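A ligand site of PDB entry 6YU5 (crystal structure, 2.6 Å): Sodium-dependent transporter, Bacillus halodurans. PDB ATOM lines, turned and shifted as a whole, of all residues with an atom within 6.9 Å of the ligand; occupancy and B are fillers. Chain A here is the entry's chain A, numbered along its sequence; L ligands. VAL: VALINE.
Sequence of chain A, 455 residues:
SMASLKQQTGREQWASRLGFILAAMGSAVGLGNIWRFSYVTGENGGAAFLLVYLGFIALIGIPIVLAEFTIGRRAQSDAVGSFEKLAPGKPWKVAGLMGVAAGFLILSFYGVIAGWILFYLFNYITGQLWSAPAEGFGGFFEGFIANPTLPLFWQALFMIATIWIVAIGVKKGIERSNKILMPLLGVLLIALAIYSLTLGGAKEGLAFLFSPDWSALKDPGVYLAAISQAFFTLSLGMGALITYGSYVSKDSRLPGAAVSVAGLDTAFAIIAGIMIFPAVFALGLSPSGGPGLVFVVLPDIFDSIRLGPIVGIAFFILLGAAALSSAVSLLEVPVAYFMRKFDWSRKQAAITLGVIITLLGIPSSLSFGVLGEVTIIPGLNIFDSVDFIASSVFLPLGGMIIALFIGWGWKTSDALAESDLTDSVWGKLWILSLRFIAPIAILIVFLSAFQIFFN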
ATOM      1  N   GLY A  26       5.220   3.398  -5.756  1.00  0.00           N
ATOM      2  CA  GLY A  26       4.815   3.157  -7.124  1.00  0.00           C
ATOM      3  C   GLY A  26       5.428   4.160  -8.093  1.00  0.00           C
ATOM      4  O   GLY A  26       5.729   3.819  -9.236  1.00  0.00           O
ATOM      5  N   SER A  27       5.604   5.401  -7.655  1.00  0.00           N
ATOM      6  CA  SER A  27       6.235   6.412  -8.498  1.00  0.00           C
ATOM      7  C   SER A  27       7.698   6.092  -8.720  1.00  0.00           C
ATOM      8  O   SER A  27       8.202   6.170  -9.843  1.00  0.00           O
ATOM      9  CB  SER A  27       6.077   7.794  -7.855  1.00  0.00           C
ATOM     10  OG  SER A  27       6.740   8.787  -8.624  1.00  0.00           O
ATOM     11  N   ALA A  28       8.411   5.713  -7.651  1.00  0.00           N
ATOM     12  CA  ALA A  28       9.855   5.538  -7.736  1.00  0.00           C
ATOM     13  C   ALA A  28      10.219   4.330  -8.598  1.00  0.00           C
ATOM     14  O   ALA A  28      11.146   4.401  -9.414  1.00  0.00           O
ATOM     15  CB  ALA A  28      10.443   5.387  -6.341  1.00  0.00           C
ATOM     16  N   VAL A  29       9.513   3.220  -8.436  1.00  0.00           N
ATOM     17  CA  VAL A  29       9.845   1.969  -9.112  1.00  0.00           C
ATOM     18  C   VAL A  29       9.188   1.956 -10.484  1.00  0.00           C
ATOM     19  O   VAL A  29       7.962   2.062 -10.609  1.00  0.00           O
ATOM     20  CB  VAL A  29       9.413   0.756  -8.273  1.00  0.00           C
ATOM     21  CG1 VAL A  29       9.712  -0.519  -9.053  1.00  0.00           C
ATOM     22  CG2 VAL A  29      10.223   0.736  -6.980  1.00  0.00           C
ATOM     23  N   GLY A  30      10.002   1.805 -11.521  1.00  0.00           N
ATOM     24  CA  GLY A  30       9.506   1.756 -12.885  1.00  0.00           C
ATOM     25  C   GLY A  30      10.596   1.414 -13.890  1.00  0.00           C
ATOM     26  O   GLY A  30      11.411   0.526 -13.647  1.00  0.00           O
ATOM     27  N   LEU A  31      10.599   2.114 -15.026  1.00  0.00           N
ATOM     28  CA  LEU A  31      11.586   1.828 -16.061  1.00  0.00           C
ATOM     29  C   LEU A  31      12.981   2.257 -15.645  1.00  0.00           C
ATOM     30  O   LEU A  31      13.974   1.710 -16.143  1.00  0.00           O
ATOM     31  CB  LEU A  31      11.194   2.503 -17.380  1.00  0.00           C
ATOM     32  CG  LEU A  31       9.995   1.931 -18.124  1.00  0.00           C
ATOM     33  CD1 LEU A  31       9.615   2.833 -19.292  1.00  0.00           C
ATOM     34  CD2 LEU A  31      10.291   0.519 -18.616  1.00  0.00           C
ATOM     35  N   GLY A  32      13.088   3.242 -14.754  1.00  0.00           N
ATOM     36  CA  GLY A  32      14.391   3.718 -14.321  1.00  0.00           C
ATOM     37  C   GLY A  32      15.219   2.649 -13.627  1.00  0.00           C
ATOM     38  O   GLY A  32      16.457   2.719 -13.626  1.00  0.00           O
ATOM     39  N   ASN A  33      14.560   1.639 -13.050  1.00  0.00           N
ATOM     40  CA  ASN A  33      15.265   0.647 -12.246  1.00  0.00           C
ATOM     41  C   ASN A  33      15.886  -0.444 -13.101  1.00  0.00           C
ATOM     42  O   ASN A  33      16.964  -0.953 -12.770  1.00  0.00           O
ATOM     43  CB  ASN A  33      14.312   0.026 -11.225  1.00  0.00           C
ATOM     44  CG  ASN A  33      13.867   1.004 -10.171  1.00  0.00           C
ATOM     45  OD1 ASN A  33      12.968   1.813 -10.382  1.00  0.00           O
ATOM     46  ND2 ASN A  33      14.499   0.940  -8.998  1.00  0.00           N
ATOM     47  N   ILE A 106      10.510  14.509 -19.147  1.00  0.00           N
ATOM     48  CA  ILE A 106      10.752  13.114 -18.831  1.00  0.00           C
ATOM     49  C   ILE A 106       9.596  12.248 -19.325  1.00  0.00           C
ATOM     50  O   ILE A 106       9.818  11.189 -19.925  1.00  0.00           O
ATOM     51  CB  ILE A 106      11.010  12.933 -17.326  1.00  0.00           C
ATOM     52  CG1 ILE A 106      12.400  13.480 -16.965  1.00  0.00           C
ATOM     53  CG2 ILE A 106      10.891  11.475 -16.921  1.00  0.00           C
ATOM     54  CD1 ILE A 106      12.769  13.293 -15.520  1.00  0.00           C
ATOM     55  N   TYR A 110       9.682   9.026 -21.615  1.00  0.00           N
ATOM     56  CA  TYR A 110       9.274   7.910 -20.773  1.00  0.00           C
ATOM     57  C   TYR A 110       8.176   7.096 -21.458  1.00  0.00           C
ATOM     58  O   TYR A 110       8.183   5.862 -21.398  1.00  0.00           O
ATOM     59  CB  TYR A 110       8.798   8.415 -19.413  1.00  0.00           C
ATOM     60  CG  TYR A 110       8.804   7.386 -18.300  1.00  0.00           C
ATOM     61  CD1 TYR A 110       7.740   6.525 -18.115  1.00  0.00           C
ATOM     62  CD2 TYR A 110       9.878   7.304 -17.420  1.00  0.00           C
ATOM     63  CE1 TYR A 110       7.741   5.593 -17.096  1.00  0.00           C
ATOM     64  CE2 TYR A 110       9.890   6.384 -16.392  1.00  0.00           C
ATOM     65  CZ  TYR A 110       8.822   5.529 -16.230  1.00  0.00           C
ATOM     66  OH  TYR A 110       8.848   4.613 -15.205  1.00  0.00           O
ATOM     67  N   GLN A 229      21.115   9.467 -12.484  1.00  0.00           N
ATOM     68  CA  GLN A 229      20.393   8.216 -12.266  1.00  0.00           C
ATOM     69  C   GLN A 229      19.783   8.170 -10.871  1.00  0.00           C
ATOM     70  O   GLN A 229      18.703   7.600 -10.686  1.00  0.00           O
ATOM     71  CB  GLN A 229      21.332   7.029 -12.474  1.00  0.00           C
ATOM     72  CG  GLN A 229      20.672   5.669 -12.297  1.00  0.00           C
ATOM     73  CD  GLN A 229      19.571   5.405 -13.312  1.00  0.00           C
ATOM     74  OE1 GLN A 229      19.567   5.975 -14.400  1.00  0.00           O
ATOM     75  NE2 GLN A 229      18.637   4.527 -12.958  1.00  0.00           N
ATOM     76  N   PHE A 231      18.711  10.839  -8.985  1.00  0.00           N
ATOM     77  CA  PHE A 231      17.534  11.705  -8.970  1.00  0.00           C
ATOM     78  C   PHE A 231      16.413  11.133  -9.830  1.00  0.00           C
ATOM     79  O   PHE A 231      15.239  11.162  -9.442  1.00  0.00           O
ATOM     80  CB  PHE A 231      17.909  13.104  -9.469  1.00  0.00           C
ATOM     81  CG  PHE A 231      18.450  14.000  -8.397  1.00  0.00           C
ATOM     82  CD1 PHE A 231      19.756  13.874  -7.956  1.00  0.00           C
ATOM     83  CD2 PHE A 231      17.667  14.993  -7.837  1.00  0.00           C
ATOM     84  CE1 PHE A 231      20.258  14.699  -6.976  1.00  0.00           C
ATOM     85  CE2 PHE A 231      18.162  15.821  -6.851  1.00  0.00           C
ATOM     86  CZ  PHE A 231      19.466  15.672  -6.418  1.00  0.00           C
ATOM     87  N   PHE A 232      16.764  10.599 -11.006  1.00  0.00           N
ATOM     88  CA  PHE A 232      15.759  10.015 -11.903  1.00  0.00           C
ATOM     89  C   PHE A 232      15.027   8.867 -11.240  1.00  0.00           C
ATOM     90  O   PHE A 232      13.784   8.822 -11.227  1.00  0.00           O
ATOM     91  CB  PHE A 232      16.453   9.545 -13.189  1.00  0.00           C
ATOM     92  CG  PHE A 232      15.523   9.069 -14.267  1.00  0.00           C
ATOM     93  CD1 PHE A 232      15.065   7.769 -14.293  1.00  0.00           C
ATOM     94  CD2 PHE A 232      15.120   9.928 -15.285  1.00  0.00           C
ATOM     95  CE1 PHE A 232      14.218   7.330 -15.292  1.00  0.00           C
ATOM     96  CE2 PHE A 232      14.276   9.503 -16.286  1.00  0.00           C
ATOM     97  CZ  PHE A 232      13.824   8.197 -16.289  1.00  0.00           C
ATOM     98  N   THR A 233      15.766   7.920 -10.651  1.00  0.00           N
ATOM     99  CA  THR A 233      15.164   6.684 -10.163  1.00  0.00           C
ATOM    100  C   THR A 233      14.327   6.912  -8.904  1.00  0.00           C
ATOM    101  O   THR A 233      13.389   6.153  -8.636  1.00  0.00           O
ATOM    102  CB  THR A 233      16.250   5.630  -9.920  1.00  0.00           C
ATOM    103  OG1 THR A 233      15.663   4.316  -9.899  1.00  0.00           O
ATOM    104  CG2 THR A 233      16.969   5.872  -8.591  1.00  0.00           C
ATOM    105  N   LEU A 234      14.645   7.953  -8.129  1.00  0.00           N
ATOM    106  CA  LEU A 234      13.883   8.292  -6.940  1.00  0.00           C
ATOM    107  C   LEU A 234      12.797   9.325  -7.222  1.00  0.00           C
ATOM    108  O   LEU A 234      12.172   9.828  -6.277  1.00  0.00           O
ATOM    109  CB  LEU A 234      14.822   8.826  -5.848  1.00  0.00           C
ATOM    110  CG  LEU A 234      15.859   7.875  -5.266  1.00  0.00           C
ATOM    111  CD1 LEU A 234      16.775   8.622  -4.303  1.00  0.00           C
ATOM    112  CD2 LEU A 234      15.190   6.711  -4.556  1.00  0.00           C
ATOM    113  N   SER A 235      12.558   9.647  -8.501  1.00  0.00           N
ATOM    114  CA  SER A 235      11.583  10.665  -8.900  1.00  0.00           C
ATOM    115  C   SER A 235      11.902  12.025  -8.290  1.00  0.00           C
ATOM    116  O   SER A 235      11.007  12.828  -8.026  1.00  0.00           O
ATOM    117  CB  SER A 235      10.161  10.227  -8.532  1.00  0.00           C
ATOM    118  OG  SER A 235       9.917   8.884  -8.925  1.00  0.00           O
ATOM    119  N   LEU A 236      13.191  12.302  -8.069  1.00  0.00           N
ATOM    120  CA  LEU A 236      13.623  13.525  -7.414  1.00  0.00           C
ATOM    121  C   LEU A 236      13.833  14.637  -8.430  1.00  0.00           C
ATOM    122  O   LEU A 236      14.455  14.419  -9.482  1.00  0.00           O
ATOM    123  CB  LEU A 236      14.918  13.286  -6.640  1.00  0.00           C
ATOM    124  CG  LEU A 236      14.807  12.481  -5.348  1.00  0.00           C
ATOM    125  CD1 LEU A 236      16.153  12.439  -4.647  1.00  0.00           C
ATOM    126  CD2 LEU A 236      13.756  13.090  -4.458  1.00  0.00           C
ATOM    127  N   MET A 238      11.538  16.339 -10.209  1.00  0.00           N
ATOM    128  CA  MET A 238      10.520  16.510 -11.237  1.00  0.00           C
ATOM    129  C   MET A 238       9.164  16.809 -10.621  1.00  0.00           C
ATOM    130  O   MET A 238       8.115  16.518 -11.222  1.00  0.00           O
ATOM    131  CB  MET A 238      10.459  15.277 -12.143  1.00  0.00           C
ATOM    132  CG  MET A 238      10.237  13.968 -11.416  1.00  0.00           C
ATOM    133  SD  MET A 238      10.924  12.556 -12.297  1.00  0.00           S
ATOM    134  CE  MET A 238      12.657  12.736 -11.896  1.00  0.00           C
ATOM    135  N   ALA A 240       7.425  15.434  -8.431  1.00  0.00           N
ATOM    136  CA  ALA A 240       6.505  14.325  -8.214  1.00  0.00           C
ATOM    137  C   ALA A 240       6.282  14.039  -6.735  1.00  0.00           C
ATOM    138  O   ALA A 240       5.158  13.730  -6.321  1.00  0.00           O
ATOM    139  CB  ALA A 240       7.023  13.063  -8.911  1.00  0.00           C
ATOM    140  N   ASP A 265      13.450   0.987  -3.700  1.00  0.00           N
ATOM    141  CA  ASP A 265      13.864   1.319  -5.061  1.00  0.00           C
ATOM    142  C   ASP A 265      15.269   0.826  -5.353  1.00  0.00           C
ATOM    143  O   ASP A 265      15.550   0.362  -6.466  1.00  0.00           O
ATOM    144  CB  ASP A 265      13.775   2.835  -5.271  1.00  0.00           C
ATOM    145  CG  ASP A 265      14.335   3.270  -6.606  1.00  0.00           C
ATOM    146  OD1 ASP A 265      13.574   3.321  -7.592  1.00  0.00           O
ATOM    147  OD2 ASP A 265      15.563   3.554  -6.660  1.00  0.00           O
ATOM    148  N   ALA A 322       4.310  -1.394 -13.731  1.00  0.00           N
ATOM    149  CA  ALA A 322       5.178  -0.523 -12.937  1.00  0.00           C
ATOM    150  C   ALA A 322       5.501   0.770 -13.667  1.00  0.00           C
ATOM    151  O   ALA A 322       5.546   1.842 -13.056  1.00  0.00           O
ATOM    152  CB  ALA A 322       6.464  -1.275 -12.582  1.00  0.00           C
ATOM    153  N   ALA A 323       5.734   0.697 -14.983  1.00  0.00           N
ATOM    154  CA  ALA A 323       5.952   1.910 -15.767  1.00  0.00           C
ATOM    155  C   ALA A 323       4.687   2.765 -15.815  1.00  0.00           C
ATOM    156  O   ALA A 323       4.782   3.993 -15.899  1.00  0.00           O
ATOM    157  CB  ALA A 323       6.409   1.548 -17.178  1.00  0.00           C
ATOM    158  N   SER A 325       2.447   3.151 -13.370  1.00  0.00           N
ATOM    159  CA  SER A 325       2.274   3.861 -12.116  1.00  0.00           C
ATOM    160  C   SER A 325       3.298   4.977 -11.954  1.00  0.00           C
ATOM    161  O   SER A 325       3.039   5.947 -11.233  1.00  0.00           O
ATOM    162  CB  SER A 325       2.358   2.883 -10.937  1.00  0.00           C
ATOM    163  OG  SER A 325       3.610   2.219 -10.906  1.00  0.00           O
ATOM    164  N   SER A 326       4.464   4.859 -12.593  1.00  0.00           N
ATOM    165  CA  SER A 326       5.433   5.948 -12.544  1.00  0.00           C
ATOM    166  C   SER A 326       5.025   7.078 -13.480  1.00  0.00           C
ATOM    167  O   SER A 326       5.124   8.259 -13.118  1.00  0.00           O
ATOM    168  CB  SER A 326       6.824   5.430 -12.919  1.00  0.00           C
ATOM    169  OG  SER A 326       7.201   4.350 -12.086  1.00  0.00           O
ATOM    170  N   ALA A 327       4.533   6.746 -14.672  1.00  0.00           N
ATOM    171  CA  ALA A 327       4.064   7.751 -15.607  1.00  0.00           C
ATOM    172  C   ALA A 327       2.838   8.483 -15.076  1.00  0.00           C
ATOM    173  O   ALA A 327       2.618   9.657 -15.412  1.00  0.00           O
ATOM    174  CB  ALA A 327       3.747   7.110 -16.957  1.00  0.00           C
ATOM    175  N   SER A 329       2.396   9.271 -11.938  1.00  0.00           N
ATOM    176  CA  SER A 329       2.901  10.252 -10.990  1.00  0.00           C
ATOM    177  C   SER A 329       3.593  11.409 -11.702  1.00  0.00           C
ATOM    178  O   SER A 329       3.677  12.513 -11.153  1.00  0.00           O
ATOM    179  CB  SER A 329       3.860   9.588 -10.008  1.00  0.00           C
ATOM    180  OG  SER A 329       4.959   9.009 -10.685  1.00  0.00           O
ATOM    181  N   LEU A 330       4.084  11.166 -12.922  1.00  0.00           N
ATOM    182  CA  LEU A 330       4.691  12.245 -13.695  1.00  0.00           C
ATOM    183  C   LEU A 330       3.644  13.206 -14.231  1.00  0.00           C
ATOM    184  O   LEU A 330       3.767  14.422 -14.076  1.00  0.00           O
ATOM    185  CB  LEU A 330       5.528  11.647 -14.830  1.00  0.00           C
ATOM    186  CG  LEU A 330       6.807  10.939 -14.392  1.00  0.00           C
ATOM    187  CD1 LEU A 330       7.349  10.094 -15.534  1.00  0.00           C
ATOM    188  CD2 LEU A 330       7.850  11.942 -13.942  1.00  0.00           C
HETATM  189  N   VAL L   1      11.443   7.451 -10.869  1.00  0.00           N
HETATM  190  CA  VAL L   1      10.647   6.677 -11.825  1.00  0.00           C
HETATM  191  C   VAL L   1      11.526   5.621 -12.501  1.00  0.00           C
HETATM  192  O   VAL L   1      12.565   5.205 -11.924  1.00  0.00           O
HETATM  193  CB  VAL L   1      10.028   7.595 -12.877  1.00  0.00           C
HETATM  194  CG1 VAL L   1       8.891   8.401 -12.261  1.00  0.00           C
HETATM  195  CG2 VAL L   1      11.092   8.549 -13.397  1.00  0.00           C
HETATM  196  OXT VAL L   1      11.200   5.165 -13.627  1.00  0.00           O
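Merely in contact with the ligand: Ser 27 (3.2 Å), Ser 326 (3.7 Å), Asn 33 (3.7 Å), Gly 30 (3.8 Å) and Leu 330 (3.9 Å).
Hydrophobic or aromatic side chains that line the ligand: Tyr 110, Phe 232 and Leu 330.
The nearest printed residue that does not touch the ligand is Met 238 (4.2 Å).
A nitrogen (N) of the ligand is in hydrogen-bond range of the backbone carbonyl oxygen (O) of Phe 232 (2.7 Å).
A nitrogen (N) of the ligand sits close to the backbone NH of Ser 235, at 3.4 Å.
N of the ligand is in hydrogen-bond range of OG of Ser 235 (2.9 Å).
The side-chain hydroxyl (OH) of Tyr 110 sits at hydrogen-bond distance from an oxygen (OXT) of the ligand, 2.9 Å away.
The backbone NH (N) of Gly 32 is in hydrogen-bond range of an oxygen (OXT) of the ligand (2.9 Å).
N of the ligand sits close to O of Ala 28 (3.4 Å).
O of Thr 233 sits at hydrogen-bond distance from N of the ligand, at 3.2 Å.
The backbone NH of Leu 31 is in hydrogen-bond range of an oxygen (OXT) of the ligand (3.4 Å).
The side-chain hydroxyl (OG) of Ser 27 lies within hydrogen-bond range of the side-chain hydroxyl (OG) of Ser 235.
The side-chain hydroxyl of Tyr 110 sits at hydrogen-bond distance from the backbone NH of Leu 31 (3.1 Å).
The backbone carbonyl oxygen of Gly 32 sits at hydrogen-bond distance from the side-chain amide nitrogen of Gln 229 (2.9 Å).
O of Ser 27 lies within hydrogen-bond range of OG of Ser 326 (3.1 Å).
The side-chain hydroxyl of Ser 27 is in hydrogen-bond range of the side-chain hydroxyl of Ser 329 (2.7 Å).
O of Ser 326 sits at hydrogen-bond distance from OG of Ser 329 (2.6 Å).
OG of Ser 326 is in hydrogen-bond range of O of Val 29 (2.8 Å).
ND2 of Asn 33 lies within hydrogen-bond range of O of Asp 265 (2.8 Å).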
